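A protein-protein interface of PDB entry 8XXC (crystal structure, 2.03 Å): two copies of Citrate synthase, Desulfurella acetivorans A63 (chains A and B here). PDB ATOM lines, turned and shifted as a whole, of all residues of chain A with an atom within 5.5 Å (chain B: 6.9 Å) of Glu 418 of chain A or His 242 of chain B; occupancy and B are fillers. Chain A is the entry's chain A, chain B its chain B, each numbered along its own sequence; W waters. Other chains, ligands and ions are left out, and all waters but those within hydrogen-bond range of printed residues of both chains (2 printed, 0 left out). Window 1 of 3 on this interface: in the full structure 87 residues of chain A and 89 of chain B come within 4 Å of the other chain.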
ATOM      1  N   MET A  42       6.149 -31.944  20.919  1.00  0.00           N
ATOM      2  CA  MET A  42       5.153 -31.915  19.856  1.00  0.00           C
ATOM      3  C   MET A  42       5.766 -32.182  18.484  1.00  0.00           C
ATOM      4  O   MET A  42       5.218 -31.747  17.475  1.00  0.00           O
ATOM      5  CB  MET A  42       4.473 -30.546  19.822  1.00  0.00           C
ATOM      6  CG  MET A  42       3.521 -30.324  20.950  1.00  0.00           C
ATOM      7  SD  MET A  42       2.740 -28.686  20.853  1.00  0.00           S
ATOM      8  CE  MET A  42       1.888 -28.649  22.427  1.00  0.00           C
ATOM      9  N   LEU A  48      -0.994 -26.451  13.944  1.00  0.00           N
ATOM     10  CA  LEU A  48      -0.878 -25.000  13.789  1.00  0.00           C
ATOM     11  C   LEU A  48      -1.242 -24.657  12.350  1.00  0.00           C
ATOM     12  O   LEU A  48      -0.863 -25.395  11.443  1.00  0.00           O
ATOM     13  CB  LEU A  48       0.563 -24.558  14.107  1.00  0.00           C
ATOM     14  CG  LEU A  48       0.944 -24.540  15.595  1.00  0.00           C
ATOM     15  CD1 LEU A  48       2.387 -24.110  15.795  1.00  0.00           C
ATOM     16  CD2 LEU A  48       0.034 -23.632  16.387  1.00  0.00           C
ATOM     17  N   HIS A 242       5.948 -19.241  17.170  1.00  0.00           N
ATOM     18  CA  HIS A 242       4.952 -19.921  17.968  1.00  0.00           C
ATOM     19  C   HIS A 242       4.717 -19.157  19.270  1.00  0.00           C
ATOM     20  O   HIS A 242       3.581 -19.002  19.743  1.00  0.00           O
ATOM     21  CB  HIS A 242       5.380 -21.384  18.110  1.00  0.00           C
ATOM     22  CG  HIS A 242       4.411 -22.216  18.849  1.00  0.00           C
ATOM     23  ND1 HIS A 242       4.796 -23.374  19.498  1.00  0.00           N
ATOM     24  CD2 HIS A 242       3.132 -22.021  19.135  1.00  0.00           C
ATOM     25  CE1 HIS A 242       3.733 -23.881  20.116  1.00  0.00           C
ATOM     26  NE2 HIS A 242       2.711 -23.090  19.879  1.00  0.00           N
ATOM     27  N   HIS A 245       2.558 -16.228  18.724  1.00  0.00           N
ATOM     28  CA  HIS A 245       1.217 -16.667  18.365  1.00  0.00           C
ATOM     29  C   HIS A 245       0.476 -17.069  19.634  1.00  0.00           C
ATOM     30  O   HIS A 245      -0.667 -16.682  19.892  1.00  0.00           O
ATOM     31  CB  HIS A 245       1.358 -17.843  17.394  1.00  0.00           C
ATOM     32  CG  HIS A 245       0.103 -18.570  17.085  1.00  0.00           C
ATOM     33  ND1 HIS A 245      -0.232 -19.794  17.648  1.00  0.00           N
ATOM     34  CD2 HIS A 245      -0.912 -18.199  16.319  1.00  0.00           C
ATOM     35  CE1 HIS A 245      -1.424 -20.152  17.185  1.00  0.00           C
ATOM     36  NE2 HIS A 245      -1.866 -19.191  16.386  1.00  0.00           N
ATOM     37  N   LEU A 246       1.151 -17.892  20.417  1.00  0.00           N
ATOM     38  CA  LEU A 246       0.593 -18.352  21.675  1.00  0.00           C
ATOM     39  C   LEU A 246       0.137 -17.162  22.502  1.00  0.00           C
ATOM     40  O   LEU A 246      -1.040 -17.048  22.848  1.00  0.00           O
ATOM     41  CB  LEU A 246       1.684 -19.205  22.300  1.00  0.00           C
ATOM     42  CG  LEU A 246       1.426 -19.692  23.735  1.00  0.00           C
ATOM     43  CD1 LEU A 246       0.062 -20.327  23.921  1.00  0.00           C
ATOM     44  CD2 LEU A 246       2.476 -20.685  24.094  1.00  0.00           C
ATOM     45  N   SER A 249      -2.675 -15.032  21.142  1.00  0.00           N
ATOM     46  CA  SER A 249      -3.895 -15.805  21.171  1.00  0.00           C
ATOM     47  C   SER A 249      -4.720 -15.546  22.436  1.00  0.00           C
ATOM     48  O   SER A 249      -5.956 -15.700  22.431  1.00  0.00           O
ATOM     49  CB  SER A 249      -3.515 -17.241  21.050  1.00  0.00           C
ATOM     50  OG  SER A 249      -4.593 -17.982  20.540  1.00  0.00           O
ATOM     51  N   ALA A 416      -8.622 -18.953  18.011  1.00  0.00           N
ATOM     52  CA  ALA A 416      -8.903 -19.079  19.438  1.00  0.00           C
ATOM     53  C   ALA A 416      -7.615 -19.119  20.248  1.00  0.00           C
ATOM     54  O   ALA A 416      -6.534 -19.396  19.728  1.00  0.00           O
ATOM     55  CB  ALA A 416      -9.712 -20.329  19.688  1.00  0.00           C
ATOM     56  N   ILE A 417      -7.789 -18.937  21.549  1.00  0.00           N
ATOM     57  CA  ILE A 417      -6.729 -19.056  22.515  1.00  0.00           C
ATOM     58  C   ILE A 417      -6.125 -20.447  22.352  1.00  0.00           C
ATOM     59  O   ILE A 417      -6.858 -21.401  22.193  1.00  0.00           O
ATOM     60  CB  ILE A 417      -7.242 -18.753  23.949  1.00  0.00           C
ATOM     61  CG1 ILE A 417      -6.060 -18.631  24.912  1.00  0.00           C
ATOM     62  CG2 ILE A 417      -8.304 -19.736  24.439  1.00  0.00           C
ATOM     63  CD1 ILE A 417      -6.427 -18.639  26.378  1.00  0.00           C
ATOM     64  N   GLU A 418      -4.791 -20.539  22.347  1.00  0.00           N
ATOM     65  CA  GLU A 418      -4.138 -21.827  22.247  1.00  0.00           C
ATOM     66  C   GLU A 418      -4.074 -22.433  23.645  1.00  0.00           C
ATOM     67  O   GLU A 418      -3.552 -21.813  24.582  1.00  0.00           O
ATOM     68  CB  GLU A 418      -2.783 -21.680  21.574  1.00  0.00           C
ATOM     69  CG  GLU A 418      -2.025 -22.967  21.510  1.00  0.00           C
ATOM     70  CD  GLU A 418      -0.695 -22.857  20.809  1.00  0.00           C
ATOM     71  OE1 GLU A 418      -0.702 -22.312  19.696  1.00  0.00           O
ATOM     72  OE2 GLU A 418       0.338 -23.352  21.368  1.00  0.00           O
ATOM     73  N   ARG A 419      -4.652 -23.643  23.774  1.00  0.00           N
ATOM     74  CA  ARG A 419      -4.817 -24.268  25.072  1.00  0.00           C
ATOM     75  C   ARG A 419      -4.896 -25.777  24.866  1.00  0.00           C
ATOM     76  O   ARG A 419      -5.967 -26.360  24.922  1.00  0.00           O
ATOM     77  CB  ARG A 419      -6.009 -23.573  25.733  1.00  0.00           C
ATOM     78  CG  ARG A 419      -6.417 -24.049  27.120  1.00  0.00           C
ATOM     79  CD  ARG A 419      -5.468 -24.905  27.913  1.00  0.00           C
ATOM     80  NE  ARG A 419      -5.746 -24.875  29.347  1.00  0.00           N
ATOM     81  CZ  ARG A 419      -5.276 -25.766  30.213  1.00  0.00           C
ATOM     82  NH1 ARG A 419      -4.671 -26.860  29.770  1.00  0.00           N
ATOM     83  NH2 ARG A 419      -5.450 -25.592  31.507  1.00  0.00           N
ATOM     84  N   PRO A 420      -3.766 -26.442  24.535  1.00  0.00           N
ATOM     85  CA  PRO A 420      -3.731 -27.907  24.482  1.00  0.00           C
ATOM     86  C   PRO A 420      -3.872 -28.481  25.891  1.00  0.00           C
ATOM     87  O   PRO A 420      -3.910 -27.733  26.857  1.00  0.00           O
ATOM     88  CB  PRO A 420      -2.365 -28.215  23.865  1.00  0.00           C
ATOM     89  CG  PRO A 420      -1.514 -27.017  24.287  1.00  0.00           C
ATOM     90  CD  PRO A 420      -2.457 -25.830  24.254  1.00  0.00           C
ATOM     91  N   GLY B  40      -8.482 -24.139  15.985  1.00  0.00           N
ATOM     92  CA  GLY B  40      -9.001 -23.687  17.261  1.00  0.00           C
ATOM     93  C   GLY B  40      -8.004 -23.876  18.396  1.00  0.00           C
ATOM     94  O   GLY B  40      -8.364 -24.351  19.461  1.00  0.00           O
ATOM     95  N   GLY B  41      -6.753 -23.459  18.187  1.00  0.00           N
ATOM     96  CA  GLY B  41      -5.829 -23.291  19.295  1.00  0.00           C
ATOM     97  C   GLY B  41      -5.525 -24.604  20.010  1.00  0.00           C
ATOM     98  O   GLY B  41      -5.448 -24.651  21.219  1.00  0.00           O
ATOM     99  N   MET B  42      -5.335 -25.659  19.232  1.00  0.00           N
ATOM    100  CA  MET B  42      -4.942 -26.969  19.721  1.00  0.00           C
ATOM    101  C   MET B  42      -5.907 -27.501  20.781  1.00  0.00           C
ATOM    102  O   MET B  42      -5.504 -28.286  21.634  1.00  0.00           O
ATOM    103  CB  MET B  42      -3.558 -26.877  20.356  1.00  0.00           C
ATOM    104  CG  MET B  42      -2.460 -26.512  19.411  1.00  0.00           C
ATOM    105  SD  MET B  42      -0.904 -26.743  20.268  1.00  0.00           S
ATOM    106  CE  MET B  42       0.235 -26.193  18.995  1.00  0.00           C
ATOM    107  N   ARG B  43      -7.176 -27.075  20.728  1.00  0.00           N
ATOM    108  CA  ARG B  43      -8.124 -27.330  21.791  1.00  0.00           C
ATOM    109  C   ARG B  43      -8.260 -28.824  22.066  1.00  0.00           C
ATOM    110  O   ARG B  43      -8.703 -29.560  21.206  1.00  0.00           O
ATOM    111  CB  ARG B  43      -9.471 -26.750  21.375  1.00  0.00           C
ATOM    112  CG  ARG B  43     -10.560 -26.859  22.429  1.00  0.00           C
ATOM    113  CD  ARG B  43     -11.911 -26.561  21.805  1.00  0.00           C
ATOM    114  NE  ARG B  43     -12.178 -27.494  20.709  1.00  0.00           N
ATOM    115  CZ  ARG B  43     -12.173 -27.169  19.414  1.00  0.00           C
ATOM    116  NH1 ARG B  43     -12.219 -28.125  18.498  1.00  0.00           N
ATOM    117  NH2 ARG B  43     -12.080 -25.896  19.047  1.00  0.00           N
ATOM    118  N   LEU B  48       1.266 -32.343  25.706  1.00  0.00           N
ATOM    119  CA  LEU B  48       2.183 -31.783  26.687  1.00  0.00           C
ATOM    120  C   LEU B  48       2.246 -32.710  27.900  1.00  0.00           C
ATOM    121  O   LEU B  48       1.241 -33.301  28.295  1.00  0.00           O
ATOM    122  CB  LEU B  48       1.673 -30.419  27.165  1.00  0.00           C
ATOM    123  CG  LEU B  48       1.822 -29.247  26.206  1.00  0.00           C
ATOM    124  CD1 LEU B  48       1.135 -28.032  26.786  1.00  0.00           C
ATOM    125  CD2 LEU B  48       3.289 -28.967  25.926  1.00  0.00           C
ATOM    126  N   GLU B 235      -1.883 -27.221  35.523  1.00  0.00           N
ATOM    127  CA  GLU B 235      -1.122 -27.987  34.543  1.00  0.00           C
ATOM    128  C   GLU B 235      -0.377 -27.077  33.561  1.00  0.00           C
ATOM    129  O   GLU B 235      -0.216 -25.888  33.818  1.00  0.00           O
ATOM    130  CB  GLU B 235      -1.998 -29.065  33.906  1.00  0.00           C
ATOM    131  CG  GLU B 235      -3.102 -28.567  33.025  1.00  0.00           C
ATOM    132  CD  GLU B 235      -3.947 -29.682  32.412  1.00  0.00           C
ATOM    133  OE1 GLU B 235      -4.277 -30.661  33.146  1.00  0.00           O
ATOM    134  OE2 GLU B 235      -4.299 -29.546  31.192  1.00  0.00           O
ATOM    135  N   SER B 236       0.119 -27.637  32.451  1.00  0.00           N
ATOM    136  CA  SER B 236       1.100 -26.917  31.648  1.00  0.00           C
ATOM    137  C   SER B 236       0.516 -26.364  30.347  1.00  0.00           C
ATOM    138  O   SER B 236       1.232 -25.684  29.621  1.00  0.00           O
ATOM    139  CB  SER B 236       2.318 -27.749  31.391  1.00  0.00           C
ATOM    140  OG  SER B 236       1.976 -28.916  30.645  1.00  0.00           O
ATOM    141  N   GLY B 237      -0.774 -26.591  30.053  1.00  0.00           N
ATOM    142  CA  GLY B 237      -1.307 -26.187  28.760  1.00  0.00           C
ATOM    143  C   GLY B 237      -1.965 -24.799  28.772  1.00  0.00           C
ATOM    144  O   GLY B 237      -2.267 -24.246  27.714  1.00  0.00           O
ATOM    145  N   ASN B 238      -2.183 -24.224  29.955  1.00  0.00           N
ATOM    146  CA  ASN B 238      -2.603 -22.830  30.063  1.00  0.00           C
ATOM    147  C   ASN B 238      -1.525 -21.945  29.441  1.00  0.00           C
ATOM    148  O   ASN B 238      -0.377 -22.364  29.335  1.00  0.00           O
ATOM    149  CB  ASN B 238      -2.922 -22.492  31.521  1.00  0.00           C
ATOM    150  CG  ASN B 238      -1.702 -22.316  32.401  1.00  0.00           C
ATOM    151  OD1 ASN B 238      -1.031 -21.293  32.340  1.00  0.00           O
ATOM    152  ND2 ASN B 238      -1.473 -23.242  33.320  1.00  0.00           N
ATOM    153  N   VAL B 239      -1.911 -20.728  29.018  1.00  0.00           N
ATOM    154  CA  VAL B 239      -1.105 -19.924  28.110  1.00  0.00           C
ATOM    155  C   VAL B 239       0.229 -19.526  28.758  1.00  0.00           C
ATOM    156  O   VAL B 239       1.258 -19.534  28.084  1.00  0.00           O
ATOM    157  CB  VAL B 239      -1.882 -18.690  27.611  1.00  0.00           C
ATOM    158  CG1 VAL B 239      -0.958 -17.664  26.964  1.00  0.00           C
ATOM    159  CG2 VAL B 239      -2.962 -19.095  26.636  1.00  0.00           C
ATOM    160  N   SER B 240       0.208 -19.214  30.065  1.00  0.00           N
ATOM    161  CA  SER B 240       1.372 -18.674  30.742  1.00  0.00           C
ATOM    162  C   SER B 240       2.381 -19.807  30.984  1.00  0.00           C
ATOM    163  O   SER B 240       3.554 -19.708  30.621  1.00  0.00           O
ATOM    164  CB  SER B 240       0.985 -17.912  31.992  1.00  0.00           C
ATOM    165  OG  SER B 240       0.258 -18.710  32.935  1.00  0.00           O
ATOM    166  N   ALA B 241       1.900 -20.906  31.557  1.00  0.00           N
ATOM    167  CA  ALA B 241       2.719 -22.073  31.833  1.00  0.00           C
ATOM    168  C   ALA B 241       3.302 -22.639  30.546  1.00  0.00           C
ATOM    169  O   ALA B 241       4.468 -23.024  30.492  1.00  0.00           O
ATOM    170  CB  ALA B 241       1.907 -23.116  32.566  1.00  0.00           C
ATOM    171  N   HIS B 242       2.472 -22.701  29.508  1.00  0.00           N
ATOM    172  CA  HIS B 242       2.918 -23.224  28.223  1.00  0.00           C
ATOM    173  C   HIS B 242       3.972 -22.319  27.618  1.00  0.00           C
ATOM    174  O   HIS B 242       4.942 -22.799  27.045  1.00  0.00           O
ATOM    175  CB  HIS B 242       1.721 -23.478  27.288  1.00  0.00           C
ATOM    176  CG  HIS B 242       2.040 -24.040  25.929  1.00  0.00           C
ATOM    177  ND1 HIS B 242       1.132 -23.922  24.898  1.00  0.00           N
ATOM    178  CD2 HIS B 242       3.101 -24.675  25.412  1.00  0.00           C
ATOM    179  CE1 HIS B 242       1.630 -24.490  23.813  1.00  0.00           C
ATOM    180  NE2 HIS B 242       2.808 -25.006  24.101  1.00  0.00           N
ATOM    181  N   THR B 243       3.732 -21.003  27.671  1.00  0.00           N
ATOM    182  CA  THR B 243       4.675 -20.048  27.118  1.00  0.00           C
ATOM    183  C   THR B 243       6.058 -20.228  27.738  1.00  0.00           C
ATOM    184  O   THR B 243       7.063 -20.209  27.017  1.00  0.00           O
ATOM    185  CB  THR B 243       4.182 -18.599  27.282  1.00  0.00           C
ATOM    186  OG1 THR B 243       2.995 -18.400  26.504  1.00  0.00           O
ATOM    187  CG2 THR B 243       5.224 -17.590  26.846  1.00  0.00           C
ATOM    188  N   ALA B 244       6.098 -20.364  29.073  1.00  0.00           N
ATOM    189  CA  ALA B 244       7.335 -20.542  29.802  1.00  0.00           C
ATOM    190  C   ALA B 244       8.013 -21.828  29.339  1.00  0.00           C
ATOM    191  O   ALA B 244       9.204 -21.832  29.048  1.00  0.00           O
ATOM    192  CB  ALA B 244       7.098 -20.549  31.304  1.00  0.00           C
ATOM    193  N   HIS B 245       7.231 -22.915  29.297  1.00  0.00           N
ATOM    194  CA  HIS B 245       7.702 -24.217  28.855  1.00  0.00           C
ATOM    195  C   HIS B 245       8.268 -24.099  27.429  1.00  0.00           C
ATOM    196  O   HIS B 245       9.389 -24.496  27.133  1.00  0.00           O
ATOM    197  CB  HIS B 245       6.515 -25.185  28.983  1.00  0.00           C
ATOM    198  CG  HIS B 245       6.744 -26.478  28.303  1.00  0.00           C
ATOM    199  ND1 HIS B 245       7.482 -27.479  28.886  1.00  0.00           N
ATOM    200  CD2 HIS B 245       6.412 -26.912  27.075  1.00  0.00           C
ATOM    201  CE1 HIS B 245       7.538 -28.511  28.046  1.00  0.00           C
ATOM    202  NE2 HIS B 245       6.911 -28.169  26.935  1.00  0.00           N
ATOM    203  N   LEU B 246       7.498 -23.496  26.529  1.00  0.00           N
ATOM    204  CA  LEU B 246       7.939 -23.352  25.134  1.00  0.00           C
ATOM    205  C   LEU B 246       9.296 -22.652  25.049  1.00  0.00           C
ATOM    206  O   LEU B 246      10.271 -23.200  24.548  1.00  0.00           O
ATOM    207  CB  LEU B 246       6.832 -22.571  24.420  1.00  0.00           C
ATOM    208  CG  LEU B 246       7.124 -22.065  23.008  1.00  0.00           C
ATOM    209  CD1 LEU B 246       7.617 -23.182  22.110  1.00  0.00           C
ATOM    210  CD2 LEU B 246       5.860 -21.451  22.428  1.00  0.00           C
ATOM    211  N   VAL B 247       9.367 -21.427  25.568  1.00  0.00           N
ATOM    212  CA  VAL B 247      10.576 -20.627  25.535  1.00  0.00           C
ATOM    213  C   VAL B 247      11.728 -21.371  26.213  1.00  0.00           C
ATOM    214  O   VAL B 247      12.821 -21.460  25.664  1.00  0.00           O
ATOM    215  CB  VAL B 247      10.330 -19.251  26.169  1.00  0.00           C
ATOM    216  CG1 VAL B 247      11.639 -18.488  26.346  1.00  0.00           C
ATOM    217  CG2 VAL B 247       9.338 -18.440  25.361  1.00  0.00           C
ATOM    218  N   ALA B 248      11.479 -21.918  27.408  1.00  0.00           N
ATOM    219  CA  ALA B 248      12.463 -22.718  28.109  1.00  0.00           C
ATOM    220  C   ALA B 248      12.971 -23.915  27.295  1.00  0.00           C
ATOM    221  O   ALA B 248      14.147 -24.270  27.374  1.00  0.00           O
ATOM    222  N   ALA B 261       6.147 -15.621  29.791  1.00  0.00           N
ATOM    223  CA  ALA B 261       4.930 -16.171  30.359  1.00  0.00           C
ATOM    224  C   ALA B 261       4.018 -15.060  30.849  1.00  0.00           C
ATOM    225  O   ALA B 261       2.798 -15.156  30.737  1.00  0.00           O
ATOM    226  CB  ALA B 261       5.244 -17.130  31.482  1.00  0.00           C
ATOM    227  N   VAL B 403       5.133 -23.020  37.687  1.00  0.00           N
ATOM    228  CA  VAL B 403       5.847 -22.920  36.433  1.00  0.00           C
ATOM    229  C   VAL B 403       7.347 -23.124  36.658  1.00  0.00           C
ATOM    230  O   VAL B 403       8.005 -23.857  35.904  1.00  0.00           O
ATOM    231  CB  VAL B 403       5.508 -21.617  35.684  1.00  0.00           C
ATOM    232  CG1 VAL B 403       6.348 -21.428  34.425  1.00  0.00           C
ATOM    233  CG2 VAL B 403       4.036 -21.583  35.333  1.00  0.00           C
ATOM    234  N   ASN B 406       8.156 -26.529  37.126  1.00  0.00           N
ATOM    235  CA  ASN B 406       8.007 -27.262  35.876  1.00  0.00           C
ATOM    236  C   ASN B 406       9.261 -27.124  35.010  1.00  0.00           C
ATOM    237  O   ASN B 406       9.691 -28.098  34.391  1.00  0.00           O
ATOM    238  CB  ASN B 406       6.707 -26.909  35.146  1.00  0.00           C
ATOM    239  CG  ASN B 406       6.351 -27.940  34.097  1.00  0.00           C
ATOM    240  OD1 ASN B 406       6.427 -29.144  34.354  1.00  0.00           O
ATOM    241  ND2 ASN B 406       6.027 -27.477  32.904  1.00  0.00           N
ATOM    242  N   GLU B 418      10.135 -27.591  21.806  1.00  0.00           N
ATOM    243  CA  GLU B 418       8.785 -27.721  21.299  1.00  0.00           C
ATOM    244  C   GLU B 418       8.725 -27.054  19.936  1.00  0.00           C
ATOM    245  O   GLU B 418       9.107 -25.908  19.830  1.00  0.00           O
ATOM    246  CB  GLU B 418       7.813 -27.083  22.277  1.00  0.00           C
ATOM    247  CG  GLU B 418       6.401 -27.062  21.736  1.00  0.00           C
ATOM    248  CD  GLU B 418       5.386 -26.600  22.739  1.00  0.00           C
ATOM    249  OE1 GLU B 418       5.461 -27.055  23.920  1.00  0.00           O
ATOM    250  OE2 GLU B 418       4.557 -25.792  22.355  1.00  0.00           O
ATOM    251  N   PRO B 420       6.065 -27.782  16.841  1.00  0.00           N
ATOM    252  CA  PRO B 420       5.049 -28.493  16.074  1.00  0.00           C
ATOM    253  C   PRO B 420       5.203 -28.068  14.614  1.00  0.00           C
ATOM    254  O   PRO B 420       6.121 -27.303  14.271  1.00  0.00           O
ATOM    255  CB  PRO B 420       3.729 -28.071  16.714  1.00  0.00           C
ATOM    256  CG  PRO B 420       4.009 -26.763  17.448  1.00  0.00           C
ATOM    257  CD  PRO B 420       5.508 -26.717  17.692  1.00  0.00           C
HETATM  258  O   HOH W   1      -1.240 -22.735  25.768  1.00  0.00           O
HETATM  259  O   HOH W   2       7.399 -23.978  18.656  1.00  0.00           O
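Met 42 of chain A touches Leu 48 of chain B, and with the chains exchanged Leu 48 of chain A touches Met 42 of chain B. Met 42 of chain A touches Glu 418 of chain B, and with the chains exchanged Glu 418 of chain A touches Met 42 of chain B. His 242 of chain A touches Glu 418 of chain B, and with the chains exchanged Glu 418 of chain A touches His 242 of chain B. His 242 of chain A touches Pro 420 of chain B, but with the chains exchanged Pro 420 of chain A does not touch His 242 of chain B (4.1 Å). 7 positions are printed for both chains.
Among the printed residues, pairs that only touch across the chains: Glu 418 of chain A with His 242 of chain B, His 242 of chain A with Glu 418 of chain B, Arg 419 of chain A with Gly 237 of chain B, Glu 418 of chain A with Gly 41 of chain B, Leu 246 of chain A with Thr 243 of chain B, Pro 420 of chain A with Met 42 of chain B, Glu 418 of chain A with Val 239 of chain B, Arg 419 of chain A with Asn 238 of chain B, Ile 417 of chain A with Val 239 of chain B, Leu 48 of chain A with Pro 420 of chain B, Met 42 of chain A with Pro 420 of chain B, Pro 420 of chain A with Gly 237 of chain B, Leu 246 of chain A with His 242 of chain B, Ile 417 of chain A with Gly 41 of chain B, Leu 48 of chain A with Met 42 of chain B, His 242 of chain A with Leu 246 of chain B, Pro 420 of chain A with Leu 48 of chain B, Met 42 of chain A with Leu 48 of chain B, Arg 419 of chain A with Met 42 of chain B, Leu 246 of chain A with Leu 246 of chain B, His 242 of chain A with Pro 420 of chain B, Arg 419 of chain A with Arg 43 of chain B, Ala 416 of chain A with Gly 41 of chain B and Met 42 of chain A with Met 42 of chain B.
The backbone carbonyl oxygen (O) of Gly 41 of chain B sits at hydrogen-bond distance from the backbone NH (N) of Arg 419 of chain A. SD of Met 42 of chain A lies close to OE2 of Glu 418 of chain B (3.7 Å). OE2 of Glu 418 of chain A sits close to SD of Met 42 of chain B (3.8 Å). NH1 of Arg 419 of chain A lies within salt-bridge range of OE2 of Glu 235 of chain B, at 3.1 Å.
Water W1 lies within hydrogen-bond range of the backbone carbonyl oxygen (O) of Gly 237 of chain B, the backbone carbonyl oxygen (O) of Glu 418 of chain A and a ring nitrogen (ND1) of His 242 of chain B. Water W2 bridges ND1 of His 242 of chain A and O of Glu 418 of chain B.
Of chain B, only Gly 41 (3.3 Å), Met 42 (3.7 Å), Val 239 (3.5 Å) and His 242 (3.0 Å) come within 4 Å of Glu 418 of chain A. His 242 of chain B touches two residues of chain A. Printed residues of chain A within 4 Å of Gly 41 of chain B: Ala 416 (3.98 Å), Ile 417 (3.6 Å), Glu 418 (3.3 Å) and Arg 419 (2.9 Å). Of the printed residues of chain A, Met 42 of chain B touches Met 42, Leu 48, Glu 418, Arg 419 and Pro 420. Printed residues of chain B within 4 Å of Leu 246 of chain A: His 242, Thr 243 and Leu 246. The nearest residue of chain B that does not touch Glu 418 of chain A is Gly 237 of chain B (4.2 Å). The nearest residue of chain A that does not touch His 242 of chain B is Pro 420 of chain A (4.1 Å).
Of the 24 printed residues of chain B, 13 touch a printed residue of chain A. Of the 11 printed residues of chain A, 9 touch a printed residue of chain B. Hydrophobic or aromatic side chains of chain A that line the printed part of chain B: Met 42, Leu 48, His 242, Leu 246, Ile 417 and Pro 420. Among the printed residues, Asp or Glu carboxylates within 4 Å of a Lys or Arg side-chain nitrogen of the other chain: Arg 419 of chain A with Glu 235 of chain B (3.1 Å).
The side-chain carboxylate (OE2) of Glu 418 of chain A sits at hydrogen-bond distance from a ring nitrogen (NE2) of His 242 of chain A (2.8 Å). The backbone carbonyl oxygen (O) of Val 239 of chain B sits at hydrogen-bond distance from the side-chain hydroxyl (OG1) of Thr 243 of chain B, at 2.6 Å. OG of Ser 249 of chain A lies close to N of Ile 417 of chain A, 3.5 Å away. The side-chain amide oxygen (OD1) of Asn 238 of chain B sits at hydrogen-bond distance from the backbone NH (N) of Ala 241 of chain B. The backbone carbonyl oxygen (O) of Ser 236 of chain B sits at hydrogen-bond distance from the backbone NH (N) of His 242 of chain B, 3.2 Å away. A ring nitrogen (NE2) of His 242 of chain B is in hydrogen-bond range of the side-chain carboxylate of Glu 418 of chain B, 2.6 Å away.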
